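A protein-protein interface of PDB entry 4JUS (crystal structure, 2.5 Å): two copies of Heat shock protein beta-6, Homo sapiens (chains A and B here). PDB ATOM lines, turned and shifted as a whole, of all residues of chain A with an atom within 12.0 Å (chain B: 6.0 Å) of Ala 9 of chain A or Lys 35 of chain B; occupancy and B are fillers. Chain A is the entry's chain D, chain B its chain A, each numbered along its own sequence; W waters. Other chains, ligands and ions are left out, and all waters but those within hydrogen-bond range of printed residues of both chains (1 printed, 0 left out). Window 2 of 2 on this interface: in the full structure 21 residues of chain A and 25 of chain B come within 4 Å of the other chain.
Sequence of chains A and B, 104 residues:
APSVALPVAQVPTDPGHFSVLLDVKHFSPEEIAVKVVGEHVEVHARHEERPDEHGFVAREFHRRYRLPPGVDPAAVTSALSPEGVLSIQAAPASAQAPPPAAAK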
ATOM      1  N   VAL A   4      -0.238 -30.392 -20.933  1.00  0.00           N
ATOM      2  CA  VAL A   4      -0.506 -29.005 -20.587  1.00  0.00           C
ATOM      3  C   VAL A   4       0.043 -28.065 -21.663  1.00  0.00           C
ATOM      4  O   VAL A   4       1.232 -28.124 -22.011  1.00  0.00           O
ATOM      5  CB  VAL A   4       0.011 -28.648 -19.177  1.00  0.00           C
ATOM      6  CG1 VAL A   4      -0.880 -29.299 -18.129  1.00  0.00           C
ATOM      7  CG2 VAL A   4       1.460 -29.090 -18.998  1.00  0.00           C
ATOM      8  N   ALA A   5      -0.850 -27.238 -22.210  1.00  0.00           N
ATOM      9  CA  ALA A   5      -0.496 -26.264 -23.247  1.00  0.00           C
ATOM     10  C   ALA A   5       0.724 -25.421 -22.852  1.00  0.00           C
ATOM     11  O   ALA A   5       0.927 -25.121 -21.676  1.00  0.00           O
ATOM     12  CB  ALA A   5      -1.702 -25.360 -23.575  1.00  0.00           C
ATOM     13  N   LEU A   6       1.533 -25.072 -23.842  1.00  0.00           N
ATOM     14  CA  LEU A   6       2.755 -24.311 -23.647  1.00  0.00           C
ATOM     15  C   LEU A   6       2.622 -23.014 -24.409  1.00  0.00           C
ATOM     16  O   LEU A   6       2.095 -22.998 -25.529  1.00  0.00           O
ATOM     17  CB  LEU A   6       3.965 -25.042 -24.238  1.00  0.00           C
ATOM     18  CG  LEU A   6       4.687 -26.175 -23.521  1.00  0.00           C
ATOM     19  CD1 LEU A   6       6.027 -26.464 -24.211  1.00  0.00           C
ATOM     20  CD2 LEU A   6       4.912 -25.814 -22.095  1.00  0.00           C
ATOM     21  N   PRO A   7       3.134 -21.921 -23.831  1.00  0.00           N
ATOM     22  CA  PRO A   7       3.136 -20.649 -24.565  1.00  0.00           C
ATOM     23  C   PRO A   7       4.137 -20.714 -25.715  1.00  0.00           C
ATOM     24  O   PRO A   7       5.215 -21.314 -25.581  1.00  0.00           O
ATOM     25  CB  PRO A   7       3.584 -19.636 -23.514  1.00  0.00           C
ATOM     26  CG  PRO A   7       4.404 -20.448 -22.539  1.00  0.00           C
ATOM     27  CD  PRO A   7       3.777 -21.819 -22.508  1.00  0.00           C
ATOM     28  N   VAL A   8       3.748 -20.126 -26.844  1.00  0.00           N
ATOM     29  CA  VAL A   8       4.591 -20.032 -28.030  1.00  0.00           C
ATOM     30  C   VAL A   8       4.965 -18.569 -28.239  1.00  0.00           C
ATOM     31  O   VAL A   8       4.086 -17.693 -28.296  1.00  0.00           O
ATOM     32  CB  VAL A   8       3.852 -20.566 -29.266  1.00  0.00           C
ATOM     33  CG1 VAL A   8       4.714 -20.428 -30.516  1.00  0.00           C
ATOM     34  CG2 VAL A   8       3.461 -22.020 -29.040  1.00  0.00           C
ATOM     35  N   ALA A   9       6.261 -18.293 -28.334  1.00  0.00           N
ATOM     36  CA  ALA A   9       6.705 -16.907 -28.421  1.00  0.00           C
ATOM     37  C   ALA A   9       6.494 -16.346 -29.832  1.00  0.00           C
ATOM     38  O   ALA A   9       6.399 -17.099 -30.798  1.00  0.00           O
ATOM     39  CB  ALA A   9       8.149 -16.772 -27.975  1.00  0.00           C
ATOM     40  N   GLN A  10       6.391 -15.025 -29.935  1.00  0.00           N
ATOM     41  CA  GLN A  10       6.141 -14.368 -31.209  1.00  0.00           C
ATOM     42  C   GLN A  10       7.104 -13.196 -31.434  1.00  0.00           C
ATOM     43  O   GLN A  10       7.603 -12.585 -30.488  1.00  0.00           O
ATOM     44  CB  GLN A  10       4.693 -13.864 -31.287  1.00  0.00           C
ATOM     45  CG  GLN A  10       3.600 -14.902 -30.989  1.00  0.00           C
ATOM     46  CD  GLN A  10       3.341 -15.914 -32.127  1.00  0.00           C
ATOM     47  OE1 GLN A  10       3.767 -15.726 -33.277  1.00  0.00           O
ATOM     48  NE2 GLN A  10       2.633 -16.999 -31.795  1.00  0.00           N
ATOM     49  N   VAL A  11       7.364 -12.884 -32.698  1.00  0.00           N
ATOM     50  CA  VAL A  11       8.133 -11.702 -33.048  1.00  0.00           C
ATOM     51  C   VAL A  11       7.165 -10.532 -33.078  1.00  0.00           C
ATOM     52  O   VAL A  11       6.032 -10.690 -33.523  1.00  0.00           O
ATOM     53  CB  VAL A  11       8.824 -11.885 -34.421  1.00  0.00           C
ATOM     54  CG1 VAL A  11       9.309 -10.539 -35.005  1.00  0.00           C
ATOM     55  CG2 VAL A  11       9.960 -12.887 -34.293  1.00  0.00           C
ATOM     56  N   PRO A  12       7.584  -9.365 -32.563  1.00  0.00           N
ATOM     57  CA  PRO A  12       6.680  -8.195 -32.516  1.00  0.00           C
ATOM     58  C   PRO A  12       6.441  -7.500 -33.863  1.00  0.00           C
ATOM     59  O   PRO A  12       7.277  -7.598 -34.754  1.00  0.00           O
ATOM     60  CB  PRO A  12       7.390  -7.234 -31.558  1.00  0.00           C
ATOM     61  CG  PRO A  12       8.827  -7.665 -31.567  1.00  0.00           C
ATOM     62  CD  PRO A  12       8.822  -9.147 -31.792  1.00  0.00           C
ATOM     63  N   THR A  13       5.314  -6.801 -33.989  1.00  0.00           N
ATOM     64  CA  THR A  13       5.007  -5.997 -35.184  1.00  0.00           C
ATOM     65  C   THR A  13       5.377  -4.510 -35.036  1.00  0.00           C
ATOM     66  O   THR A  13       6.177  -4.144 -34.176  1.00  0.00           O
ATOM     67  CB  THR A  13       3.529  -6.090 -35.532  1.00  0.00           C
ATOM     68  OG1 THR A  13       2.776  -6.251 -34.318  1.00  0.00           O
ATOM     69  CG2 THR A  13       3.281  -7.279 -36.462  1.00  0.00           C
ATOM     70  N   ALA B  33      11.893 -12.496 -28.984  1.00  0.00           N
ATOM     71  CA  ALA B  33      10.692 -13.254 -28.718  1.00  0.00           C
ATOM     72  C   ALA B  33       9.979 -12.724 -27.475  1.00  0.00           C
ATOM     73  O   ALA B  33      10.597 -12.493 -26.434  1.00  0.00           O
ATOM     74  CB  ALA B  33      11.026 -14.747 -28.579  1.00  0.00           C
ATOM     75  N   VAL B  34       8.676 -12.523 -27.619  1.00  0.00           N
ATOM     76  CA  VAL B  34       7.818 -12.023 -26.567  1.00  0.00           C
ATOM     77  C   VAL B  34       6.698 -13.028 -26.366  1.00  0.00           C
ATOM     78  O   VAL B  34       6.071 -13.458 -27.335  1.00  0.00           O
ATOM     79  CB  VAL B  34       7.171 -10.675 -26.960  1.00  0.00           C
ATOM     80  CG1 VAL B  34       6.229 -10.209 -25.857  1.00  0.00           C
ATOM     81  CG2 VAL B  34       8.234  -9.639 -27.243  1.00  0.00           C
ATOM     82  N   LYS B  35       6.433 -13.389 -25.116  1.00  0.00           N
ATOM     83  CA  LYS B  35       5.343 -14.306 -24.816  1.00  0.00           C
ATOM     84  C   LYS B  35       4.772 -14.111 -23.403  1.00  0.00           C
ATOM     85  O   LYS B  35       5.469 -13.694 -22.474  1.00  0.00           O
ATOM     86  CB  LYS B  35       5.796 -15.761 -25.011  1.00  0.00           C
ATOM     87  CG  LYS B  35       7.025 -16.140 -24.200  1.00  0.00           C
ATOM     88  CD  LYS B  35       7.302 -17.638 -24.226  1.00  0.00           C
ATOM     89  CE  LYS B  35       8.476 -17.977 -23.314  1.00  0.00           C
ATOM     90  NZ  LYS B  35       8.883 -19.398 -23.372  1.00  0.00           N
ATOM     91  N   VAL B  36       3.491 -14.415 -23.248  1.00  0.00           N
ATOM     92  CA  VAL B  36       2.873 -14.385 -21.931  1.00  0.00           C
ATOM     93  C   VAL B  36       2.954 -15.779 -21.307  1.00  0.00           C
ATOM     94  O   VAL B  36       2.600 -16.767 -21.936  1.00  0.00           O
ATOM     95  CB  VAL B  36       1.408 -13.887 -21.989  1.00  0.00           C
ATOM     96  CG1 VAL B  36       0.862 -13.680 -20.584  1.00  0.00           C
ATOM     97  CG2 VAL B  36       1.325 -12.585 -22.772  1.00  0.00           C
ATOM     98  N   VAL B  37       3.464 -15.845 -20.082  1.00  0.00           N
ATOM     99  CA  VAL B  37       3.536 -17.087 -19.338  1.00  0.00           C
ATOM    100  C   VAL B  37       2.779 -16.926 -18.020  1.00  0.00           C
ATOM    101  O   VAL B  37       3.275 -16.314 -17.069  1.00  0.00           O
ATOM    102  CB  VAL B  37       4.987 -17.474 -19.051  1.00  0.00           C
ATOM    103  CG1 VAL B  37       5.053 -18.875 -18.434  1.00  0.00           C
ATOM    104  CG2 VAL B  37       5.816 -17.370 -20.324  1.00  0.00           C
ATOM    105  N   HIS B  40       2.962 -13.645 -16.223  1.00  0.00           N
ATOM    106  CA  HIS B  40       4.155 -12.903 -16.607  1.00  0.00           C
ATOM    107  C   HIS B  40       4.272 -12.659 -18.112  1.00  0.00           C
ATOM    108  O   HIS B  40       3.786 -13.450 -18.923  1.00  0.00           O
ATOM    109  CB  HIS B  40       5.407 -13.629 -16.130  1.00  0.00           C
ATOM    110  CG  HIS B  40       5.570 -13.649 -14.645  1.00  0.00           C
ATOM    111  ND1 HIS B  40       4.954 -14.583 -13.842  1.00  0.00           N
ATOM    112  CD2 HIS B  40       6.290 -12.856 -13.819  1.00  0.00           C
ATOM    113  CE1 HIS B  40       5.285 -14.363 -12.581  1.00  0.00           C
ATOM    114  NE2 HIS B  40       6.097 -13.321 -12.542  1.00  0.00           N
ATOM    115  N   VAL B  41       4.919 -11.549 -18.472  1.00  0.00           N
ATOM    116  CA  VAL B  41       5.332 -11.297 -19.849  1.00  0.00           C
ATOM    117  C   VAL B  41       6.834 -11.480 -19.945  1.00  0.00           C
ATOM    118  O   VAL B  41       7.579 -10.932 -19.148  1.00  0.00           O
ATOM    119  CB  VAL B  41       4.991  -9.881 -20.311  1.00  0.00           C
ATOM    120  CG1 VAL B  41       5.770  -9.552 -21.553  1.00  0.00           C
ATOM    121  CG2 VAL B  41       3.504  -9.752 -20.584  1.00  0.00           C
ATOM    122  N   GLU B  42       7.285 -12.263 -20.914  1.00  0.00           N
ATOM    123  CA  GLU B  42       8.713 -12.492 -21.075  1.00  0.00           C
ATOM    124  C   GLU B  42       9.226 -11.989 -22.418  1.00  0.00           C
ATOM    125  O   GLU B  42       8.536 -12.045 -23.442  1.00  0.00           O
ATOM    126  CB  GLU B  42       9.056 -13.965 -20.888  1.00  0.00           C
ATOM    127  CG  GLU B  42       8.478 -14.535 -19.616  1.00  0.00           C
ATOM    128  CD  GLU B  42       8.889 -15.963 -19.369  1.00  0.00           C
ATOM    129  OE1 GLU B  42       9.667 -16.510 -20.180  1.00  0.00           O
ATOM    130  OE2 GLU B  42       8.435 -16.533 -18.359  1.00  0.00           O
ATOM    131  N   VAL B  43      10.451 -11.483 -22.387  1.00  0.00           N
ATOM    132  CA  VAL B  43      11.091 -10.950 -23.560  1.00  0.00           C
ATOM    133  C   VAL B  43      12.460 -11.558 -23.601  1.00  0.00           C
ATOM    134  O   VAL B  43      13.197 -11.497 -22.615  1.00  0.00           O
ATOM    135  CB  VAL B  43      11.237  -9.419 -23.481  1.00  0.00           C
ATOM    136  CG1 VAL B  43      11.862  -8.893 -24.742  1.00  0.00           C
ATOM    137  CG2 VAL B  43       9.893  -8.778 -23.259  1.00  0.00           C
HETATM  138  O   HOH W   1       7.716 -21.866 -25.249  1.00  0.00           O
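O of Val 34 of chain B sits at hydrogen-bond distance from N of Gln 10 of chain A (3.1 Å).
The backbone carbonyl oxygen (O) of Lys 35 of chain B is in hydrogen-bond range of the backbone NH (N) of Glu 42 of chain B.
O of Val 36 of chain B touches CB of Pro 7 of chain A (3.4 Å). Ala 33 of chain B touches Ala 9 of chain A (CB to CB, 3.6 Å). Ala 9 of chain A touches Val 34 of chain B (CA to O, 3.7 Å). CA of Ala 9 of chain A touches CB of Lys 35 of chain B, at 3.7 Å. CA of Ala 33 of chain B touches O of Gln 10 of chain A, at 3.6 Å.
Of the printed residues of chain B, Pro 7 of chain A touches Val 36 (3.4 Å). Ala 9 of chain A touches just these residues of chain B: Ala 33, Val 34 and Lys 35. Printed residues of chain B within 4 Å of Gln 10 of chain A: Ala 33 (3.6 Å) and Val 34 (3.1 Å). Val 11 of chain A touches none of the printed residues of chain B. Val 34 of chain B touches two residues of chain A. Lys 35 of chain B touches just one residue of chain A: Ala 9 (3.7 Å). Of chain A, only Pro 7 (3.4 Å) comes within 4 Å of Val 36 of chain B. No residue of chain A comes within 4 Å of Val 37 of chain B. His 40 of chain B touches none of the printed residues of chain A. No residue of chain A comes within 4 Å of Val 41 of chain B. Glu 42 of chain B touches none of the printed residues of chain A. No residue of chain A comes within 4 Å of Val 43 of chain B. The nearest residue of chain A that does not touch Lys 35 of chain B is Val 8 of chain A (4.2 Å).
Printed residues of chain B that touch a printed residue of chain A: Ala 33, Val 34, Lys 35 and Val 36. Of the 10 printed residues of chain A, 3 touch a printed residue of chain B. Printed residues of chain A that touch a printed residue of chain B: Pro 7, Ala 9 and Gln 10.
No position is printed for both chains.
Water W1 bridges O of Pro 7 of chain A and NZ of Lys 35 of chain B.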
